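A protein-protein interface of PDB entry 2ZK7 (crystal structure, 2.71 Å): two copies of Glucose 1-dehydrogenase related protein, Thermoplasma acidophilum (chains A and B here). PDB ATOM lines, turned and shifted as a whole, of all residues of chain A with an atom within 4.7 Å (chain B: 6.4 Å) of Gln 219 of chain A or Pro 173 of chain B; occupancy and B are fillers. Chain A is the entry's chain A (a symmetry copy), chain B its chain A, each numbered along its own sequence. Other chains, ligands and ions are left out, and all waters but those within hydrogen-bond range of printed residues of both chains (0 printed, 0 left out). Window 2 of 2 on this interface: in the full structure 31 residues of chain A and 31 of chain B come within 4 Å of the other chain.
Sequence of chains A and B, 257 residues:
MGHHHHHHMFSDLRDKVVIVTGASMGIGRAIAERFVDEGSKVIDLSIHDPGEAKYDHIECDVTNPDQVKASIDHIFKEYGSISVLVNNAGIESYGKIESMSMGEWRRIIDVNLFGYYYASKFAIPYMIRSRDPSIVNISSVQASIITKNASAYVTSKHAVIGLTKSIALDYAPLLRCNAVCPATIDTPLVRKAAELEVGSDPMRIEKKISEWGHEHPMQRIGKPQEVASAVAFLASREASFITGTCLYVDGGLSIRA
NE2 of Gln 219 of chain A lies within hydrogen-bond range of O of His 216 of chain A (3.5 Å).
O of Pro 217 of chain A sits at hydrogen-bond distance from NE2 of Gln 219 of chain A, 3.4 Å away.
Among the printed residues, pairs that only touch across the chains: Pro 217 of chain A with Ala 172 of chain B, Met 218 of chain A with Pro 173 of chain B, Pro 217 of chain A with Pro 173 of chain B and Gln 219 of chain A with Pro 173 of chain B.
Of chain B, only Pro 173 (3.6 Å) comes within 4 Å of Gln 219 of chain A.
Of the printed residues of chain A, Pro 173 of chain B touches Pro 217 (3.5 Å), Met 218 (3.3 Å) and Gln 219 (3.6 Å).
Of the printed residues of chain A, Ala 172 of chain B touches Pro 217.
Printed residues of chain B within 4 Å of Pro 217 of chain A: Ala 172 (3.2 Å) and Pro 173 (3.5 Å).
The nearest residue of chain B that does not touch Gln 219 of chain A is Ala 172 of chain B (5.4 Å).
The nearest printed residue of chain A that does not touch Pro 173 of chain B is Arg 220 of chain A (6.2 Å).
Hydrophobic or aromatic side chains of chain B within 4 Å of the printed part of chain A: Ala 172 and Pro 173.
Hydrophobic or aromatic side chains of chain A within 4 Å of the printed part of chain B: Pro 217.
Along chain A the printed residues that touch a printed residue of chain B span positions 217 to 219.
No position is printed for both chains.
Of the 4 pairs that touch across the chains among the printed residues, none has its exchanged pair printed and touching as well.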
ATOM      1  N   GLY A 213      11.242 -13.314   1.885  1.00  0.00           N
ATOM      2  CA  GLY A 213      12.194 -14.057   1.080  1.00  0.00           C
ATOM      3  C   GLY A 213      12.094 -13.712  -0.391  1.00  0.00           C
ATOM      4  O   GLY A 213      13.098 -13.693  -1.097  1.00  0.00           O
ATOM      5  N   HIS A 214      10.880 -13.419  -0.846  1.00  0.00           N
ATOM      6  CA  HIS A 214      10.638 -13.126  -2.253  1.00  0.00           C
ATOM      7  C   HIS A 214      11.056 -11.718  -2.675  1.00  0.00           C
ATOM      8  O   HIS A 214      11.136 -11.422  -3.868  1.00  0.00           O
ATOM      9  CB  HIS A 214       9.186 -13.429  -2.617  1.00  0.00           C
ATOM     10  CG  HIS A 214       8.905 -14.892  -2.758  1.00  0.00           C
ATOM     11  ND1 HIS A 214       9.159 -15.799  -1.751  1.00  0.00           N
ATOM     12  CD2 HIS A 214       8.402 -15.608  -3.791  1.00  0.00           C
ATOM     13  CE1 HIS A 214       8.822 -17.010  -2.156  1.00  0.00           C
ATOM     14  NE2 HIS A 214       8.360 -16.922  -3.390  1.00  0.00           N
ATOM     15  N   HIS A 216      14.017 -10.774  -1.828  1.00  0.00           N
ATOM     16  CA  HIS A 216      15.330 -11.234  -2.259  1.00  0.00           C
ATOM     17  C   HIS A 216      15.175 -11.994  -3.576  1.00  0.00           C
ATOM     18  O   HIS A 216      14.278 -12.832  -3.706  1.00  0.00           O
ATOM     19  CB  HIS A 216      15.958 -12.140  -1.189  1.00  0.00           C
ATOM     20  CG  HIS A 216      16.220 -11.447   0.115  1.00  0.00           C
ATOM     21  ND1 HIS A 216      15.223 -11.165   1.025  1.00  0.00           N
ATOM     22  CD2 HIS A 216      17.369 -10.984   0.664  1.00  0.00           C
ATOM     23  CE1 HIS A 216      15.744 -10.555   2.074  1.00  0.00           C
ATOM     24  NE2 HIS A 216      17.045 -10.432   1.881  1.00  0.00           N
ATOM     25  N   PRO A 217      16.032 -11.686  -4.567  1.00  0.00           N
ATOM     26  CA  PRO A 217      16.062 -12.437  -5.826  1.00  0.00           C
ATOM     27  C   PRO A 217      16.200 -13.951  -5.639  1.00  0.00           C
ATOM     28  O   PRO A 217      15.821 -14.712  -6.526  1.00  0.00           O
ATOM     29  CB  PRO A 217      17.299 -11.872  -6.533  1.00  0.00           C
ATOM     30  CG  PRO A 217      17.417 -10.491  -6.009  1.00  0.00           C
ATOM     31  CD  PRO A 217      17.003 -10.577  -4.573  1.00  0.00           C
ATOM     32  N   MET A 218      16.728 -14.369  -4.489  1.00  0.00           N
ATOM     33  CA  MET A 218      16.948 -15.781  -4.182  1.00  0.00           C
ATOM     34  C   MET A 218      15.706 -16.451  -3.597  1.00  0.00           C
ATOM     35  O   MET A 218      15.776 -17.594  -3.133  1.00  0.00           O
ATOM     36  CB  MET A 218      18.110 -15.935  -3.206  1.00  0.00           C
ATOM     37  CG  MET A 218      19.468 -15.471  -3.722  1.00  0.00           C
ATOM     38  SD  MET A 218      20.569 -16.784  -4.302  1.00  0.00           S
ATOM     39  CE  MET A 218      20.472 -17.972  -2.962  1.00  0.00           C
ATOM     40  N   GLN A 219      14.583 -15.731  -3.613  1.00  0.00           N
ATOM     41  CA  GLN A 219      13.271 -16.228  -3.160  1.00  0.00           C
ATOM     42  C   GLN A 219      13.252 -16.781  -1.719  1.00  0.00           C
ATOM     43  O   GLN A 219      12.382 -17.584  -1.364  1.00  0.00           O
ATOM     44  CB  GLN A 219      12.692 -17.251  -4.153  1.00  0.00           C
ATOM     45  CG  GLN A 219      12.703 -16.813  -5.623  1.00  0.00           C
ATOM     46  CD  GLN A 219      11.822 -15.609  -5.907  1.00  0.00           C
ATOM     47  OE1 GLN A 219      10.595 -15.707  -5.905  1.00  0.00           O
ATOM     48  NE2 GLN A 219      12.450 -14.466  -6.172  1.00  0.00           N
ATOM     49  N   ARG A 220      14.210 -16.342  -0.902  1.00  0.00           N
ATOM     50  CA  ARG A 220      14.314 -16.753   0.500  1.00  0.00           C
ATOM     51  C   ARG A 220      15.211 -15.807   1.291  1.00  0.00           C
ATOM     52  O   ARG A 220      16.116 -15.183   0.738  1.00  0.00           O
ATOM     53  CB  ARG A 220      14.841 -18.192   0.628  1.00  0.00           C
ATOM     54  CG  ARG A 220      16.268 -18.391   0.129  1.00  0.00           C
ATOM     55  CD  ARG A 220      16.889 -19.649   0.693  1.00  0.00           C
ATOM     56  NE  ARG A 220      18.219 -19.897   0.135  1.00  0.00           N
ATOM     57  CZ  ARG A 220      19.368 -19.563   0.722  1.00  0.00           C
ATOM     58  NH1 ARG A 220      20.517 -19.841   0.125  1.00  0.00           N
ATOM     59  NH2 ARG A 220      19.380 -18.955   1.904  1.00  0.00           N
ATOM     60  N   ALA B 168      22.985 -12.499 -12.490  1.00  0.00           N
ATOM     61  CA  ALA B 168      22.632 -12.884 -11.147  1.00  0.00           C
ATOM     62  C   ALA B 168      21.192 -12.526 -10.844  1.00  0.00           C
ATOM     63  O   ALA B 168      20.522 -13.217 -10.072  1.00  0.00           O
ATOM     64  CB  ALA B 168      23.559 -12.262 -10.153  1.00  0.00           C
ATOM     65  N   LEU B 169      20.703 -11.458 -11.463  1.00  0.00           N
ATOM     66  CA  LEU B 169      19.311 -11.046 -11.258  1.00  0.00           C
ATOM     67  C   LEU B 169      18.350 -11.968 -12.000  1.00  0.00           C
ATOM     68  O   LEU B 169      17.391 -12.461 -11.412  1.00  0.00           O
ATOM     69  CB  LEU B 169      19.090  -9.587 -11.677  1.00  0.00           C
ATOM     70  CG  LEU B 169      17.793  -8.943 -11.185  1.00  0.00           C
ATOM     71  CD1 LEU B 169      17.845  -8.691  -9.688  1.00  0.00           C
ATOM     72  CD2 LEU B 169      17.515  -7.638 -11.932  1.00  0.00           C
ATOM     73  N   ASP B 170      18.619 -12.204 -13.283  1.00  0.00           N
ATOM     74  CA  ASP B 170      17.756 -13.023 -14.128  1.00  0.00           C
ATOM     75  C   ASP B 170      17.637 -14.473 -13.670  1.00  0.00           C
ATOM     76  O   ASP B 170      16.593 -15.094 -13.870  1.00  0.00           O
ATOM     77  CB  ASP B 170      18.278 -13.047 -15.565  1.00  0.00           C
ATOM     78  CG  ASP B 170      18.034 -11.753 -16.319  1.00  0.00           C
ATOM     79  OD1 ASP B 170      17.409 -10.812 -15.783  1.00  0.00           O
ATOM     80  OD2 ASP B 170      18.485 -11.692 -17.482  1.00  0.00           O
ATOM     81  N   TYR B 171      18.699 -15.009 -13.066  1.00  0.00           N
ATOM     82  CA  TYR B 171      18.815 -16.448 -12.853  1.00  0.00           C
ATOM     83  C   TYR B 171      18.797 -16.915 -11.394  1.00  0.00           C
ATOM     84  O   TYR B 171      18.954 -18.112 -11.117  1.00  0.00           O
ATOM     85  CB  TYR B 171      20.026 -16.996 -13.618  1.00  0.00           C
ATOM     86  CG  TYR B 171      19.874 -16.823 -15.110  1.00  0.00           C
ATOM     87  CD1 TYR B 171      20.493 -15.764 -15.778  1.00  0.00           C
ATOM     88  CD2 TYR B 171      19.081 -17.705 -15.858  1.00  0.00           C
ATOM     89  CE1 TYR B 171      20.343 -15.596 -17.152  1.00  0.00           C
ATOM     90  CE2 TYR B 171      18.919 -17.542 -17.234  1.00  0.00           C
ATOM     91  CZ  TYR B 171      19.554 -16.487 -17.872  1.00  0.00           C
ATOM     92  OH  TYR B 171      19.399 -16.322 -19.230  1.00  0.00           O
ATOM     93  N   ALA B 172      18.602 -15.983 -10.465  1.00  0.00           N
ATOM     94  CA  ALA B 172      18.326 -16.348  -9.080  1.00  0.00           C
ATOM     95  C   ALA B 172      16.881 -16.827  -9.035  1.00  0.00           C
ATOM     96  O   ALA B 172      16.057 -16.349  -9.815  1.00  0.00           O
ATOM     97  CB  ALA B 172      18.521 -15.163  -8.168  1.00  0.00           C
ATOM     98  N   PRO B 173      16.561 -17.780  -8.141  1.00  0.00           N
ATOM     99  CA  PRO B 173      17.433 -18.476  -7.200  1.00  0.00           C
ATOM    100  C   PRO B 173      18.048 -19.735  -7.802  1.00  0.00           C
ATOM    101  O   PRO B 173      18.597 -20.567  -7.071  1.00  0.00           O
ATOM    102  CB  PRO B 173      16.467 -18.872  -6.087  1.00  0.00           C
ATOM    103  CG  PRO B 173      15.200 -19.138  -6.803  1.00  0.00           C
ATOM    104  CD  PRO B 173      15.163 -18.229  -8.010  1.00  0.00           C
ATOM    105  N   LEU B 174      17.942 -19.875  -9.119  1.00  0.00           N
ATOM    106  CA  LEU B 174      18.431 -21.063  -9.796  1.00  0.00           C
ATOM    107  C   LEU B 174      19.960 -21.129  -9.775  1.00  0.00           C
ATOM    108  O   LEU B 174      20.545 -22.154  -9.447  1.00  0.00           O
ATOM    109  CB  LEU B 174      17.875 -21.126 -11.223  1.00  0.00           C
ATOM    110  CG  LEU B 174      16.348 -21.296 -11.340  1.00  0.00           C
ATOM    111  CD1 LEU B 174      15.869 -21.085 -12.774  1.00  0.00           C
ATOM    112  CD2 LEU B 174      15.878 -22.656 -10.799  1.00  0.00           C
ATOM    113  N   LEU B 175      20.600 -20.011 -10.081  1.00  0.00           N
ATOM    114  CA  LEU B 175      22.038 -19.973 -10.262  1.00  0.00           C
ATOM    115  C   LEU B 175      22.590 -18.694  -9.639  1.00  0.00           C
ATOM    116  O   LEU B 175      21.934 -17.652  -9.685  1.00  0.00           O
ATOM    117  CB  LEU B 175      22.347 -20.050 -11.764  1.00  0.00           C
ATOM    118  CG  LEU B 175      23.750 -19.789 -12.301  1.00  0.00           C
ATOM    119  CD1 LEU B 175      24.049 -20.705 -13.482  1.00  0.00           C
ATOM    120  CD2 LEU B 175      23.879 -18.318 -12.685  1.00  0.00           C
ATOM    121  N   ARG B 176      23.779 -18.789  -9.047  1.00  0.00           N
ATOM    122  CA  ARG B 176      24.494 -17.628  -8.501  1.00  0.00           C
ATOM    123  C   ARG B 176      25.556 -17.145  -9.475  1.00  0.00           C
ATOM    124  O   ARG B 176      26.185 -17.944 -10.162  1.00  0.00           O
ATOM    125  CB  ARG B 176      25.169 -17.973  -7.176  1.00  0.00           C
ATOM    126  CG  ARG B 176      24.230 -18.174  -5.998  1.00  0.00           C
ATOM    127  CD  ARG B 176      24.994 -18.513  -4.720  1.00  0.00           C
ATOM    128  NE  ARG B 176      25.891 -19.660  -4.890  1.00  0.00           N
ATOM    129  CZ  ARG B 176      27.223 -19.593  -4.924  1.00  0.00           C
ATOM    130  NH1 ARG B 176      27.848 -18.431  -4.796  1.00  0.00           N
ATOM    131  NH2 ARG B 176      27.934 -20.700  -5.083  1.00  0.00           N
